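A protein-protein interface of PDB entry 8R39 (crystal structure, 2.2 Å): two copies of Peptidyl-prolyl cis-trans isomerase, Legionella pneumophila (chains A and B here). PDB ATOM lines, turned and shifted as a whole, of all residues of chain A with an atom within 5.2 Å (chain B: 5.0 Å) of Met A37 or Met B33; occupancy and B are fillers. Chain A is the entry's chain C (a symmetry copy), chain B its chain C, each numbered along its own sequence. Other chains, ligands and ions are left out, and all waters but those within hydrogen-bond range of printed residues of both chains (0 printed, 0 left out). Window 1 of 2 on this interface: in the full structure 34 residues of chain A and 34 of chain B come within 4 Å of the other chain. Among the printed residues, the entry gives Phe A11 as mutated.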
ATOM      1  N   SER A  10     -12.643  -2.579  19.487  1.00  0.00           N
ATOM      2  CA  SER A  10     -13.669  -2.604  18.423  1.00  0.00           C
ATOM      3  C   SER A  10     -15.051  -2.852  19.040  1.00  0.00           C
ATOM      4  O   SER A  10     -15.986  -2.123  18.688  1.00  0.00           O
ATOM      5  CB  SER A  10     -13.301  -3.622  17.387  1.00  0.00           C
ATOM      6  OG  SER A  10     -12.130  -3.243  16.682  1.00  0.00           O
ATOM      7  N   PHE A  11     -15.150  -3.790  19.973  1.00  0.00           N
ATOM      8  CA  PHE A  11     -16.427  -4.137  20.640  1.00  0.00           C
ATOM      9  C   PHE A  11     -16.892  -2.972  21.471  1.00  0.00           C
ATOM     10  O   PHE A  11     -18.093  -2.699  21.489  1.00  0.00           O
ATOM     11  CB  PHE A  11     -16.176  -5.376  21.497  1.00  0.00           C
ATOM     12  CG  PHE A  11     -17.331  -5.787  22.393  1.00  0.00           C
ATOM     13  CD1 PHE A  11     -17.555  -5.149  23.603  1.00  0.00           C
ATOM     14  CD2 PHE A  11     -18.185  -6.813  22.021  1.00  0.00           C
ATOM     15  CE1 PHE A  11     -18.611  -5.522  24.412  1.00  0.00           C
ATOM     16  CE2 PHE A  11     -19.236  -7.185  22.836  1.00  0.00           C
ATOM     17  CZ  PHE A  11     -19.447  -6.540  24.029  1.00  0.00           C
ATOM     18  N   ILE A  13     -16.263   0.239  21.061  1.00  0.00           N
ATOM     19  CA  ILE A  13     -16.734   1.347  20.183  1.00  0.00           C
ATOM     20  C   ILE A  13     -18.151   1.006  19.700  1.00  0.00           C
ATOM     21  O   ILE A  13     -19.019   1.884  19.768  1.00  0.00           O
ATOM     22  CB  ILE A  13     -15.752   1.588  19.022  1.00  0.00           C
ATOM     23  CG1 ILE A  13     -14.432   2.175  19.512  1.00  0.00           C
ATOM     24  CG2 ILE A  13     -16.389   2.466  17.945  1.00  0.00           C
ATOM     25  CD1 ILE A  13     -13.257   1.916  18.590  1.00  0.00           C
ATOM     26  N   GLY A  14     -18.375  -0.234  19.279  1.00  0.00           N
ATOM     27  CA  GLY A  14     -19.688  -0.672  18.788  1.00  0.00           C
ATOM     28  C   GLY A  14     -20.744  -0.546  19.855  1.00  0.00           C
ATOM     29  O   GLY A  14     -21.857  -0.116  19.525  1.00  0.00           O
ATOM     30  N   ALA A  15     -20.416  -0.891  21.092  1.00  0.00           N
ATOM     31  CA  ALA A  15     -21.380  -0.857  22.207  1.00  0.00           C
ATOM     32  C   ALA A  15     -21.798   0.585  22.476  1.00  0.00           C
ATOM     33  O   ALA A  15     -22.988   0.821  22.698  1.00  0.00           O
ATOM     34  CB  ALA A  15     -20.753  -1.491  23.410  1.00  0.00           C
ATOM     35  N   LEU A  17     -21.772   3.112  20.334  1.00  0.00           N
ATOM     36  CA  LEU A  17     -22.615   3.535  19.192  1.00  0.00           C
ATOM     37  C   LEU A  17     -24.025   2.976  19.384  1.00  0.00           C
ATOM     38  O   LEU A  17     -24.977   3.730  19.184  1.00  0.00           O
ATOM     39  CB  LEU A  17     -21.995   3.035  17.893  1.00  0.00           C
ATOM     40  CG  LEU A  17     -20.711   3.732  17.449  1.00  0.00           C
ATOM     41  CD1 LEU A  17     -19.853   2.795  16.634  1.00  0.00           C
ATOM     42  CD2 LEU A  17     -21.041   4.977  16.665  1.00  0.00           C
ATOM     43  N   MET A  33     -23.665  -2.290   8.279  1.00  0.00           N
ATOM     44  CA  MET A  33     -22.707  -1.243   8.700  1.00  0.00           C
ATOM     45  C   MET A  33     -21.298  -1.833   8.636  1.00  0.00           C
ATOM     46  O   MET A  33     -20.401  -1.144   8.150  1.00  0.00           O
ATOM     47  CB  MET A  33     -23.001  -0.764  10.121  1.00  0.00           C
ATOM     48  CG  MET A  33     -22.218   0.456  10.536  1.00  0.00           C
ATOM     49  SD  MET A  33     -22.532   0.912  12.251  1.00  0.00           S
ATOM     50  CE  MET A  33     -24.001   1.923  12.050  1.00  0.00           C
ATOM     51  N   ALA A  34     -21.129  -3.069   9.093  1.00  0.00           N
ATOM     52  CA  ALA A  34     -19.818  -3.751   9.085  1.00  0.00           C
ATOM     53  C   ALA A  34     -19.326  -3.907   7.649  1.00  0.00           C
ATOM     54  O   ALA A  34     -18.134  -3.716   7.416  1.00  0.00           O
ATOM     55  CB  ALA A  34     -19.928  -5.076   9.772  1.00  0.00           C
ATOM     56  N   LYS A  35     -20.227  -4.221   6.725  1.00  0.00           N
ATOM     57  CA  LYS A  35     -19.855  -4.400   5.302  1.00  0.00           C
ATOM     58  C   LYS A  35     -19.275  -3.083   4.769  1.00  0.00           C
ATOM     59  O   LYS A  35     -18.203  -3.127   4.168  1.00  0.00           O
ATOM     60  CB  LYS A  35     -21.074  -4.865   4.504  1.00  0.00           C
ATOM     61  CG  LYS A  35     -20.919  -4.908   2.996  1.00  0.00           C
ATOM     62  CD  LYS A  35     -19.928  -5.957   2.520  1.00  0.00           C
ATOM     63  CE  LYS A  35     -20.092  -6.243   1.066  1.00  0.00           C
ATOM     64  NZ  LYS A  35     -18.847  -6.756   0.497  1.00  0.00           N
ATOM     65  N   GLY A  36     -19.956  -1.965   5.001  1.00  0.00           N
ATOM     66  CA  GLY A  36     -19.508  -0.652   4.508  1.00  0.00           C
ATOM     67  C   GLY A  36     -18.188  -0.252   5.123  1.00  0.00           C
ATOM     68  O   GLY A  36     -17.339   0.267   4.386  1.00  0.00           O
ATOM     69  N   MET A  37     -18.018  -0.499   6.417  1.00  0.00           N
ATOM     70  CA  MET A  37     -16.759  -0.176   7.125  1.00  0.00           C
ATOM     71  C   MET A  37     -15.620  -1.000   6.518  1.00  0.00           C
ATOM     72  O   MET A  37     -14.558  -0.423   6.252  1.00  0.00           O
ATOM     73  CB  MET A  37     -16.897  -0.483   8.616  1.00  0.00           C
ATOM     74  CG  MET A  37     -15.741   0.016   9.450  1.00  0.00           C
ATOM     75  SD  MET A  37     -15.950  -0.292  11.213  1.00  0.00           S
ATOM     76  CE  MET A  37     -17.494   0.578  11.507  1.00  0.00           C
ATOM     77  N   GLN A  38     -15.852  -2.287   6.280  1.00  0.00           N
ATOM     78  CA  GLN A  38     -14.823  -3.198   5.724  1.00  0.00           C
ATOM     79  C   GLN A  38     -14.457  -2.756   4.307  1.00  0.00           C
ATOM     80  O   GLN A  38     -13.258  -2.617   4.041  1.00  0.00           O
ATOM     81  CB  GLN A  38     -15.352  -4.628   5.715  1.00  0.00           C
ATOM     82  CG  GLN A  38     -14.314  -5.684   5.359  1.00  0.00           C
ATOM     83  CD  GLN A  38     -13.424  -6.041   6.527  1.00  0.00           C
ATOM     84  OE1 GLN A  38     -13.739  -6.924   7.331  1.00  0.00           O
ATOM     85  NE2 GLN A  38     -12.302  -5.347   6.633  1.00  0.00           N
ATOM     86  N   ASP A  39     -15.446  -2.510   3.455  1.00  0.00           N
ATOM     87  CA  ASP A  39     -15.192  -2.184   2.028  1.00  0.00           C
ATOM     88  C   ASP A  39     -14.443  -0.855   1.933  1.00  0.00           C
ATOM     89  O   ASP A  39     -13.550  -0.751   1.079  1.00  0.00           O
ATOM     90  CB  ASP A  39     -16.483  -2.242   1.237  1.00  0.00           C
ATOM     91  CG  ASP A  39     -17.144  -3.610   1.167  1.00  0.00           C
ATOM     92  OD1 ASP A  39     -16.422  -4.623   1.216  1.00  0.00           O
ATOM     93  OD2 ASP A  39     -18.376  -3.650   1.076  1.00  0.00           O
ATOM     94  N   ALA A  40     -14.754   0.100   2.800  1.00  0.00           N
ATOM     95  CA  ALA A  40     -14.088   1.420   2.804  1.00  0.00           C
ATOM     96  C   ALA A  40     -12.626   1.263   3.210  1.00  0.00           C
ATOM     97  O   ALA A  40     -11.776   1.907   2.588  1.00  0.00           O
ATOM     98  CB  ALA A  40     -14.808   2.352   3.735  1.00  0.00           C
ATOM     99  N   MET A  41     -12.340   0.410   4.184  1.00  0.00           N
ATOM    100  CA  MET A  41     -10.966   0.242   4.717  1.00  0.00           C
ATOM    101  C   MET A  41     -10.135  -0.625   3.762  1.00  0.00           C
ATOM    102  O   MET A  41      -8.940  -0.344   3.625  1.00  0.00           O
ATOM    103  CB  MET A  41     -11.044  -0.392   6.108  1.00  0.00           C
ATOM    104  CG  MET A  41     -11.877   0.408   7.085  1.00  0.00           C
ATOM    105  SD  MET A  41     -11.604  -0.032   8.811  1.00  0.00           S
ATOM    106  CE  MET A  41     -10.012   0.759   9.068  1.00  0.00           C
ATOM    107  N   SER A  42     -10.749  -1.624   3.130  1.00  0.00           N
ATOM    108  CA  SER A  42     -10.072  -2.547   2.181  1.00  0.00           C
ATOM    109  C   SER A  42      -9.708  -1.819   0.882  1.00  0.00           C
ATOM    110  O   SER A  42      -8.799  -2.294   0.186  1.00  0.00           O
ATOM    111  CB  SER A  42     -10.950  -3.729   1.905  1.00  0.00           C
ATOM    112  OG  SER A  42     -11.984  -3.396   0.993  1.00  0.00           O
ATOM    113  N   GLY B  14     -21.396   3.126   8.056  1.00  0.00           N
ATOM    114  CA  GLY B  14     -20.200   2.284   8.197  1.00  0.00           C
ATOM    115  C   GLY B  14     -19.089   2.752   7.293  1.00  0.00           C
ATOM    116  O   GLY B  14     -17.937   2.760   7.742  1.00  0.00           O
ATOM    117  N   ALA B  15     -19.414   3.144   6.068  1.00  0.00           N
ATOM    118  CA  ALA B  15     -18.406   3.573   5.081  1.00  0.00           C
ATOM    119  C   ALA B  15     -17.738   4.858   5.561  1.00  0.00           C
ATOM    120  O   ALA B  15     -16.516   4.969   5.434  1.00  0.00           O
ATOM    121  CB  ALA B  15     -19.075   3.754   3.753  1.00  0.00           C
ATOM    122  N   LEU B  17     -17.435   5.913   8.686  1.00  0.00           N
ATOM    123  CA  LEU B  17     -16.587   5.549   9.845  1.00  0.00           C
ATOM    124  C   LEU B  17     -15.285   4.935   9.330  1.00  0.00           C
ATOM    125  O   LEU B  17     -14.229   5.309   9.840  1.00  0.00           O
ATOM    126  CB  LEU B  17     -17.342   4.573  10.738  1.00  0.00           C
ATOM    127  CG  LEU B  17     -18.509   5.155  11.533  1.00  0.00           C
ATOM    128  CD1 LEU B  17     -19.551   4.095  11.800  1.00  0.00           C
ATOM    129  CD2 LEU B  17     -18.009   5.754  12.824  1.00  0.00           C
ATOM    130  N   GLY B  18     -15.373   4.049   8.345  1.00  0.00           N
ATOM    131  CA  GLY B  18     -14.199   3.351   7.811  1.00  0.00           C
ATOM    132  C   GLY B  18     -13.216   4.327   7.223  1.00  0.00           C
ATOM    133  O   GLY B  18     -12.027   4.208   7.529  1.00  0.00           O
ATOM    134  N   PHE B  21     -11.446   6.252  10.035  1.00  0.00           N
ATOM    135  CA  PHE B  21     -10.494   5.400  10.786  1.00  0.00           C
ATOM    136  C   PHE B  21      -9.264   5.143   9.944  1.00  0.00           C
ATOM    137  O   PHE B  21      -8.162   5.159  10.495  1.00  0.00           O
ATOM    138  CB  PHE B  21     -11.128   4.056  11.146  1.00  0.00           C
ATOM    139  CG  PHE B  21     -12.133   4.029  12.288  1.00  0.00           C
ATOM    140  CD1 PHE B  21     -11.860   4.638  13.504  1.00  0.00           C
ATOM    141  CD2 PHE B  21     -13.336   3.352  12.148  1.00  0.00           C
ATOM    142  CE1 PHE B  21     -12.779   4.591  14.538  1.00  0.00           C
ATOM    143  CE2 PHE B  21     -14.250   3.307  13.185  1.00  0.00           C
ATOM    144  CZ  PHE B  21     -13.970   3.926  14.377  1.00  0.00           C
ATOM    145  N   VAL B  28      -9.179  -1.546  13.304  1.00  0.00           N
ATOM    146  CA  VAL B  28     -10.431  -2.007  13.962  1.00  0.00           C
ATOM    147  C   VAL B  28     -10.955  -3.283  13.298  1.00  0.00           C
ATOM    148  O   VAL B  28     -10.775  -3.399  12.079  1.00  0.00           O
ATOM    149  CB  VAL B  28     -11.451  -0.860  13.849  1.00  0.00           C
ATOM    150  CG1 VAL B  28     -12.884  -1.325  14.065  1.00  0.00           C
ATOM    151  CG2 VAL B  28     -11.117   0.292  14.782  1.00  0.00           C
ATOM    152  N   ASN B  29     -11.568  -4.186  14.065  1.00  0.00           N
ATOM    153  CA  ASN B  29     -12.218  -5.406  13.519  1.00  0.00           C
ATOM    154  C   ASN B  29     -13.707  -5.099  13.340  1.00  0.00           C
ATOM    155  O   ASN B  29     -14.404  -4.981  14.355  1.00  0.00           O
ATOM    156  CB  ASN B  29     -12.044  -6.623  14.410  1.00  0.00           C
ATOM    157  CG  ASN B  29     -12.844  -7.806  13.928  1.00  0.00           C
ATOM    158  OD1 ASN B  29     -13.174  -7.905  12.742  1.00  0.00           O
ATOM    159  ND2 ASN B  29     -13.166  -8.717  14.830  1.00  0.00           N
ATOM    160  N   PRO B  30     -14.228  -4.957  12.108  1.00  0.00           N
ATOM    161  CA  PRO B  30     -15.626  -4.608  11.929  1.00  0.00           C
ATOM    162  C   PRO B  30     -16.619  -5.606  12.515  1.00  0.00           C
ATOM    163  O   PRO B  30     -17.678  -5.179  12.978  1.00  0.00           O
ATOM    164  CB  PRO B  30     -15.708  -4.543  10.409  1.00  0.00           C
ATOM    165  CG  PRO B  30     -14.322  -4.194   9.980  1.00  0.00           C
ATOM    166  CD  PRO B  30     -13.522  -5.110  10.854  1.00  0.00           C
ATOM    167  N   GLU B  31     -16.286  -6.893  12.512  1.00  0.00           N
ATOM    168  CA  GLU B  31     -17.192  -7.956  13.009  1.00  0.00           C
ATOM    169  C   GLU B  31     -17.384  -7.828  14.520  1.00  0.00           C
ATOM    170  O   GLU B  31     -18.516  -7.999  14.982  1.00  0.00           O
ATOM    171  CB  GLU B  31     -16.623  -9.330  12.682  1.00  0.00           C
ATOM    172  CG  GLU B  31     -17.698 -10.374  12.398  1.00  0.00           C
ATOM    173  CD  GLU B  31     -18.332 -10.335  11.015  1.00  0.00           C
ATOM    174  OE1 GLU B  31     -19.325 -11.070  10.822  1.00  0.00           O
ATOM    175  OE2 GLU B  31     -17.854  -9.589  10.134  1.00  0.00           O
ATOM    176  N   ALA B  32     -16.324  -7.535  15.253  1.00  0.00           N
ATOM    177  CA  ALA B  32     -16.390  -7.388  16.718  1.00  0.00           C
ATOM    178  C   ALA B  32     -17.157  -6.113  17.068  1.00  0.00           C
ATOM    179  O   ALA B  32     -17.850  -6.100  18.089  1.00  0.00           O
ATOM    180  CB  ALA B  32     -14.993  -7.388  17.267  1.00  0.00           C
ATOM    181  N   MET B  33     -17.049  -5.083  16.237  1.00  0.00           N
ATOM    182  CA  MET B  33     -17.795  -3.823  16.450  1.00  0.00           C
ATOM    183  C   MET B  33     -19.285  -4.115  16.271  1.00  0.00           C
ATOM    184  O   MET B  33     -20.074  -3.627  17.081  1.00  0.00           O
ATOM    185  CB  MET B  33     -17.357  -2.747  15.456  1.00  0.00           C
ATOM    186  CG  MET B  33     -17.902  -1.373  15.754  1.00  0.00           C
ATOM    187  SD  MET B  33     -17.437  -0.172  14.494  1.00  0.00           S
ATOM    188  CE  MET B  33     -15.828   0.332  15.111  1.00  0.00           C
ATOM    189  N   ALA B  34     -19.639  -4.899  15.260  1.00  0.00           N
ATOM    190  CA  ALA B  34     -21.046  -5.258  14.982  1.00  0.00           C
ATOM    191  C   ALA B  34     -21.623  -6.034  16.162  1.00  0.00           C
ATOM    192  O   ALA B  34     -22.775  -5.789  16.515  1.00  0.00           O
ATOM    193  CB  ALA B  34     -21.130  -6.049  13.714  1.00  0.00           C
ATOM    194  N   LYS B  35     -20.832  -6.921  16.756  1.00  0.00           N
ATOM    195  CA  LYS B  35     -21.295  -7.730  17.908  1.00  0.00           C
ATOM    196  C   LYS B  35     -21.667  -6.789  19.061  1.00  0.00           C
ATOM    197  O   LYS B  35     -22.758  -6.949  19.606  1.00  0.00           O
ATOM    198  CB  LYS B  35     -20.211  -8.735  18.302  1.00  0.00           C
ATOM    199  CG  LYS B  35     -20.441  -9.509  19.586  1.00  0.00           C
ATOM    200  CD  LYS B  35     -21.617 -10.468  19.510  1.00  0.00           C
ATOM    201  CE  LYS B  35     -21.571 -11.474  20.609  1.00  0.00           C
ATOM    202  NZ  LYS B  35     -22.910 -11.986  20.897  1.00  0.00           N
ATOM    203  N   GLY B  36     -20.797  -5.842  19.396  1.00  0.00           N
ATOM    204  CA  GLY B  36     -21.039  -4.906  20.507  1.00  0.00           C
ATOM    205  C   GLY B  36     -22.241  -4.033  20.242  1.00  0.00           C
ATOM    206  O   GLY B  36     -23.024  -3.824  21.178  1.00  0.00           O
ATOM    207  N   MET B  37     -22.390  -3.556  19.010  1.00  0.00           N
ATOM    208  CA  MET B  37     -23.543  -2.711  18.623  1.00  0.00           C
ATOM    209  C   MET B  37     -24.831  -3.523  18.782  1.00  0.00           C
ATOM    210  O   MET B  37     -25.792  -2.990  19.352  1.00  0.00           O
ATOM    211  CB  MET B  37     -23.389  -2.239  17.178  1.00  0.00           C
ATOM    212  CG  MET B  37     -24.404  -1.198  16.767  1.00  0.00           C
ATOM    213  SD  MET B  37     -24.168  -0.600  15.083  1.00  0.00           S
ATOM    214  CE  MET B  37     -22.487   0.023  15.200  1.00  0.00           C
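Of chain B, only Gly B14 (3.2 Å), Ala B15 (3.9 Å) and Met B33 (3.1 Å) come within 4 Å of Met A37.
Of chain A, only Ser A10 (3.3 Å), Ile A13 (3.6 Å), Gly A14 (3.4 Å) and Met A37 (3.1 Å) come within 4 Å of Met B33.
Of the printed residues of chain A, Met B37 touches Gly A14 (3.2 Å), Ala A15 (3.9 Å) and Met A33 (3.1 Å).
Printed residues of chain A within 4 Å of Ala B32: Phe A11 (3.5 Å).
Printed residues of chain B within 4 Å of Met A41: Gly B18.
Of the printed residues of chain B, Gln A38 touches Pro B30.
Printed residues of chain B within 4 Å of Gly A36: Gly B14 (3.8 Å) and Ala B15 (3.5 Å).
Lys B35 touches none of the printed residues of chain A.
Ser A42 touches none of the printed residues of chain B.
The nearest residue of chain B that does not touch Met A37 is Gly B18 (4.02 Å).
The nearest printed residue of chain A that does not touch Met B33 is Leu A17 (4.4 Å).
The nearest printed residue of chain B that does not touch Ala A40 is Gly B18 (4.2 Å).
CG1 of Val B28 touches OG of Ser A10 (3.3 Å).
O of Ala B32 touches CA of Phe A11, at 3.5 Å.
CE2 of Phe A11 touches CA of Gly B36, at 3.7 Å.
Gly A14 touches Met B33 (CA to O, 3.4 Å).
Gly B36 touches Gly A14.
Gly A14 touches Met B37 (O to CA, 3.2 Å).
CA of Gly B14 touches O of Met A33, 3.4 Å away.
Gly A36 touches Gly B14.
O of Gly A36 touches CA of Ala B15, at 3.5 Å.
CA of Met A37 touches O of Gly B14, 3.2 Å away.
Of the 16 printed residues of chain A, 12 touch a printed residue of chain B.
Hydrophobic or aromatic side chains of chain A within 4 Å of the printed part of chain B: Phe A11, Ile A13, Ala A15, Met A33, Ala A34, Met A37, Ala A40 and Met A41.
Of the 15 printed residues of chain B, 10 touch a printed residue of chain A.
Hydrophobic or aromatic side chains of chain B within 4 Å of the printed part of chain A: Ala B15, Val B28, Pro B30, Met B33 and Met B37.
Among the printed residues, no Asp or Glu carboxylate lies within 4 Å of a Lys or Arg side-chain nitrogen of the other chain.
N of Asn B29 lies within hydrogen-bond range of OG of Ser A10 (2.8 Å).
SD of Met A33 sits close to SD of Met B37, 3.6 Å away.
SD of Met B33 lies close to SD of Met A37, 3.6 Å away.
Gly A14 touches Gly B36, and with the chains exchanged Gly A36 touches Gly B14.
Gly A14 touches Met B37, and with the chains exchanged Met A37 touches Gly B14.
Ala A15 touches Gly B36, and with the chains exchanged Gly A36 touches Ala B15.
Met A33 touches Met B37, and with the chains exchanged Met A37 touches Met B33.
Of the 22 pairs that touch across the chains among the printed residues, 12 have their exchanged pair printed and touching as well.
The backbone NH (N) of Glu B31 lies close to the side-chain amide oxygen (OD1) of Asn B29, 3.3 Å away.
The backbone NH (N) of Ala B32 sits close to the side-chain amide nitrogen (ND2) of Asn B29 (3.4 Å).
O of Gln A38 lies close to OG of Ser A42 (3.4 Å).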
